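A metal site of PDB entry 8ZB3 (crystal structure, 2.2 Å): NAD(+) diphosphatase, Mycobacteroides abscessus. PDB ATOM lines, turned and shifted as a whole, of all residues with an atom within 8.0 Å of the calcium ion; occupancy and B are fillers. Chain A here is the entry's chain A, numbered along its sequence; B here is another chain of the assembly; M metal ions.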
ATOM      1  N   ALA A  19      25.154  10.599  -2.207  1.00  0.00           N
ATOM      2  CA  ALA A  19      25.591   9.213  -2.099  1.00  0.00           C
ATOM      3  C   ALA A  19      26.395   9.001  -0.804  1.00  0.00           C
ATOM      4  O   ALA A  19      27.532   8.519  -0.867  1.00  0.00           O
ATOM      5  CB  ALA A  19      26.396   8.835  -3.321  1.00  0.00           C
ATOM      6  N   ASP A  20      25.778   9.346   0.318  1.00  0.00           N
ATOM      7  CA  ASP A  20      26.466   9.407   1.607  1.00  0.00           C
ATOM      8  C   ASP A  20      27.105   8.059   1.916  1.00  0.00           C
ATOM      9  O   ASP A  20      28.243   8.015   2.405  1.00  0.00           O
ATOM     10  CB  ASP A  20      25.494   9.849   2.702  1.00  0.00           C
ATOM     11  CG  ASP A  20      24.426   8.823   3.007  1.00  0.00           C
ATOM     12  OD1 ASP A  20      23.624   8.425   2.076  1.00  0.00           O
ATOM     13  OD2 ASP A  20      24.377   8.413   4.164  1.00  0.00           O
ATOM     14  N   GLU A  21      26.426   6.957   1.601  1.00  0.00           N
ATOM     15  CA  GLU A  21      26.916   5.634   1.998  1.00  0.00           C
ATOM     16  C   GLU A  21      28.254   5.324   1.329  1.00  0.00           C
ATOM     17  O   GLU A  21      29.035   4.556   1.912  1.00  0.00           O
ATOM     18  CB  GLU A  21      25.881   4.540   1.727  1.00  0.00           C
ATOM     19  CG  GLU A  21      24.698   4.637   2.672  1.00  0.00           C
ATOM     20  CD  GLU A  21      25.143   4.559   4.112  1.00  0.00           C
ATOM     21  OE1 GLU A  21      24.915   5.525   4.882  1.00  0.00           O
ATOM     22  OE2 GLU A  21      25.804   3.565   4.422  1.00  0.00           O
ATOM     23  N   LEU A  22      28.547   5.936   0.175  1.00  0.00           N
ATOM     24  CA  LEU A  22      29.819   5.673  -0.479  1.00  0.00           C
ATOM     25  C   LEU A  22      31.001   6.367   0.189  1.00  0.00           C
ATOM     26  O   LEU A  22      32.152   5.917   0.000  1.00  0.00           O
ATOM     27  CB  LEU A  22      29.758   6.112  -1.950  1.00  0.00           C
ATOM     28  CG  LEU A  22      28.845   5.274  -2.847  1.00  0.00           C
ATOM     29  CD1 LEU A  22      28.890   5.756  -4.281  1.00  0.00           C
ATOM     30  CD2 LEU A  22      29.295   3.819  -2.765  1.00  0.00           C
ATOM     31  N   ARG A  23      30.740   7.408   0.988  1.00  0.00           N
ATOM     32  CA  ARG A  23      31.803   8.121   1.668  1.00  0.00           C
ATOM     33  C   ARG A  23      32.587   7.199   2.591  1.00  0.00           C
ATOM     34  O   ARG A  23      33.809   7.353   2.722  1.00  0.00           O
ATOM     35  CB  ARG A  23      31.249   9.278   2.529  1.00  0.00           C
ATOM     36  CG  ARG A  23      30.556  10.398   1.749  1.00  0.00           C
ATOM     37  CD  ARG A  23      29.712  11.215   2.710  1.00  0.00           C
ATOM     38  NE  ARG A  23      29.064  12.326   2.046  1.00  0.00           N
ATOM     39  CZ  ARG A  23      28.254  13.206   2.638  1.00  0.00           C
ATOM     40  NH1 ARG A  23      27.976  13.087   3.928  1.00  0.00           N
ATOM     41  NH2 ARG A  23      27.745  14.205   1.943  1.00  0.00           N
ATOM     42  N   SER A  24      31.874   6.271   3.255  1.00  0.00           N
ATOM     43  CA  SER A  24      32.458   5.328   4.185  1.00  0.00           C
ATOM     44  C   SER A  24      32.817   3.999   3.519  1.00  0.00           C
ATOM     45  O   SER A  24      33.081   3.032   4.216  1.00  0.00           O
ATOM     46  CB  SER A  24      31.508   5.098   5.329  1.00  0.00           C
ATOM     47  OG  SER A  24      31.249   6.311   6.007  1.00  0.00           O
ATOM     48  N   ARG B 206      16.705  15.271   2.927  1.00  0.00           N
ATOM     49  CA  ARG B 206      17.802  14.315   2.816  1.00  0.00           C
ATOM     50  C   ARG B 206      17.805  13.392   4.050  1.00  0.00           C
ATOM     51  O   ARG B 206      17.896  12.185   3.916  1.00  0.00           O
ATOM     52  CB  ARG B 206      19.134  15.046   2.624  1.00  0.00           C
ATOM     53  CG  ARG B 206      20.348  14.143   2.598  1.00  0.00           C
ATOM     54  CD  ARG B 206      21.673  14.902   2.440  1.00  0.00           C
ATOM     55  NE  ARG B 206      21.936  15.858   3.517  1.00  0.00           N
ATOM     56  CZ  ARG B 206      22.060  15.548   4.803  1.00  0.00           C
ATOM     57  NH1 ARG B 206      22.104  14.295   5.205  1.00  0.00           N
ATOM     58  NH2 ARG B 206      22.180  16.496   5.725  1.00  0.00           N
ATOM     59  N   GLU B 207      17.720  13.993   5.244  1.00  0.00           N
ATOM     60  CA  GLU B 207      17.840  13.249   6.482  1.00  0.00           C
ATOM     61  C   GLU B 207      16.662  12.286   6.680  1.00  0.00           C
ATOM     62  O   GLU B 207      16.834  11.185   7.143  1.00  0.00           O
ATOM     63  CB  GLU B 207      17.962  14.185   7.677  1.00  0.00           C
ATOM     64  CG  GLU B 207      19.324  14.852   7.785  1.00  0.00           C
ATOM     65  CD  GLU B 207      20.479  13.960   8.221  1.00  0.00           C
ATOM     66  OE1 GLU B 207      21.610  14.413   8.153  1.00  0.00           O
ATOM     67  OE2 GLU B 207      20.255  12.810   8.588  1.00  0.00           O
ATOM     68  N   ALA B 209      14.971  10.865   4.285  1.00  0.00           N
ATOM     69  CA  ALA B 209      15.244   9.800   3.328  1.00  0.00           C
ATOM     70  C   ALA B 209      16.315   8.838   3.876  1.00  0.00           C
ATOM     71  O   ALA B 209      16.118   7.633   3.818  1.00  0.00           O
ATOM     72  CB  ALA B 209      15.646  10.373   1.979  1.00  0.00           C
ATOM     73  N   GLU B 210      17.407   9.389   4.418  1.00  0.00           N
ATOM     74  CA  GLU B 210      18.493   8.587   4.967  1.00  0.00           C
ATOM     75  C   GLU B 210      18.001   7.696   6.116  1.00  0.00           C
ATOM     76  O   GLU B 210      18.451   6.572   6.254  1.00  0.00           O
ATOM     77  CB  GLU B 210      19.615   9.448   5.540  1.00  0.00           C
ATOM     78  CG  GLU B 210      20.521  10.051   4.493  1.00  0.00           C
ATOM     79  CD  GLU B 210      21.224   9.004   3.650  1.00  0.00           C
ATOM     80  OE1 GLU B 210      21.777   8.045   4.241  1.00  0.00           O
ATOM     81  OE2 GLU B 210      21.201   9.133   2.402  1.00  0.00           O
ATOM     82  N   GLU B 211      17.102   8.202   6.964  1.00  0.00           N
ATOM     83  CA  GLU B 211      16.788   7.531   8.197  1.00  0.00           C
ATOM     84  C   GLU B 211      15.671   6.505   8.008  1.00  0.00           C
ATOM     85  O   GLU B 211      15.726   5.403   8.555  1.00  0.00           O
ATOM     86  CB  GLU B 211      16.378   8.523   9.282  1.00  0.00           C
ATOM     87  CG  GLU B 211      17.502   9.506   9.632  1.00  0.00           C
ATOM     88  CD  GLU B 211      18.702   8.872  10.330  1.00  0.00           C
ATOM     89  OE1 GLU B 211      19.826   8.965   9.770  1.00  0.00           O
ATOM     90  OE2 GLU B 211      18.526   8.310  11.425  1.00  0.00           O
ATOM     91  N   PHE B 249      15.444   1.361   6.291  1.00  0.00           N
ATOM     92  CA  PHE B 249      16.264   1.834   7.387  1.00  0.00           C
ATOM     93  C   PHE B 249      17.743   1.662   7.131  1.00  0.00           C
ATOM     94  O   PHE B 249      18.492   2.014   8.031  1.00  0.00           O
ATOM     95  CB  PHE B 249      15.912   1.050   8.641  1.00  0.00           C
ATOM     96  CG  PHE B 249      14.459   1.159   9.005  1.00  0.00           C
ATOM     97  CD1 PHE B 249      13.846   2.403   9.080  1.00  0.00           C
ATOM     98  CD2 PHE B 249      13.716   0.021   9.243  1.00  0.00           C
ATOM     99  CE1 PHE B 249      12.510   2.491   9.419  1.00  0.00           C
ATOM    100  CE2 PHE B 249      12.382   0.110   9.595  1.00  0.00           C
ATOM    101  CZ  PHE B 249      11.774   1.337   9.670  1.00  0.00           C
ATOM    102  N   ASN B 250      18.150   1.100   5.987  1.00  0.00           N
ATOM    103  CA  ASN B 250      19.539   0.671   5.836  1.00  0.00           C
ATOM    104  C   ASN B 250      20.502   1.865   5.867  1.00  0.00           C
ATOM    105  O   ASN B 250      21.425   1.796   6.652  1.00  0.00           O
ATOM    106  CB  ASN B 250      19.761  -0.352   4.712  1.00  0.00           C
ATOM    107  CG  ASN B 250      19.210   0.045   3.368  1.00  0.00           C
ATOM    108  OD1 ASN B 250      18.014   0.314   3.254  1.00  0.00           O
ATOM    109  ND2 ASN B 250      20.071   0.066   2.354  1.00  0.00           N
ATOM    110  N   ASP B 251      20.197   2.964   5.153  1.00  0.00           N
ATOM    111  CA  ASP B 251      21.125   4.073   5.009  1.00  0.00           C
ATOM    112  C   ASP B 251      21.272   4.887   6.315  1.00  0.00           C
ATOM    113  O   ASP B 251      22.093   5.776   6.355  1.00  0.00           O
ATOM    114  CB  ASP B 251      20.679   4.979   3.865  1.00  0.00           C
ATOM    115  CG  ASP B 251      21.092   4.533   2.468  1.00  0.00           C
ATOM    116  OD1 ASP B 251      21.203   3.299   2.239  1.00  0.00           O
ATOM    117  OD2 ASP B 251      21.294   5.432   1.604  1.00  0.00           O
ATOM    118  N   GLY B 252      20.501   4.598   7.362  1.00  0.00           N
ATOM    119  CA  GLY B 252      20.403   5.477   8.518  1.00  0.00           C
ATOM    120  C   GLY B 252      20.755   4.806   9.834  1.00  0.00           C
ATOM    121  O   GLY B 252      21.313   3.710   9.830  1.00  0.00           O
ATOM    122  N   GLU B 253      20.366   5.432  10.941  1.00  0.00           N
ATOM    123  CA  GLU B 253      20.635   4.936  12.281  1.00  0.00           C
ATOM    124  C   GLU B 253      19.330   4.535  12.957  1.00  0.00           C
ATOM    125  O   GLU B 253      19.297   4.497  14.179  1.00  0.00           O
ATOM    126  CB  GLU B 253      21.352   5.993  13.131  1.00  0.00           C
ATOM    127  CG  GLU B 253      22.883   5.841  13.116  1.00  0.00           C
ATOM    128  CD  GLU B 253      23.543   6.327  11.838  1.00  0.00           C
ATOM    129  OE1 GLU B 253      23.309   7.503  11.502  1.00  0.00           O
ATOM    130  OE2 GLU B 253      24.246   5.541  11.164  1.00  0.00           O
HETATM  131 CA    CA M   1      23.534   7.171   5.395  1.00  0.00          CA
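The calcium ion is bound by the side-chain carboxylate of Asp 20, the side-chain carboxylate of Glu 21, the backbone carbonyl oxygen of Asp 251 of chain B and the side-chain carboxylate of Glu 210 of chain B.
The side-chain carboxylate of Asp 251 of chain B sits at hydrogen-bond distance from the side-chain amide nitrogen of Asn 250 of chain B (3.4 Å).
O of Glu 210 of chain B lies within hydrogen-bond range of N of Gly 252 of chain B (3.1 Å).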
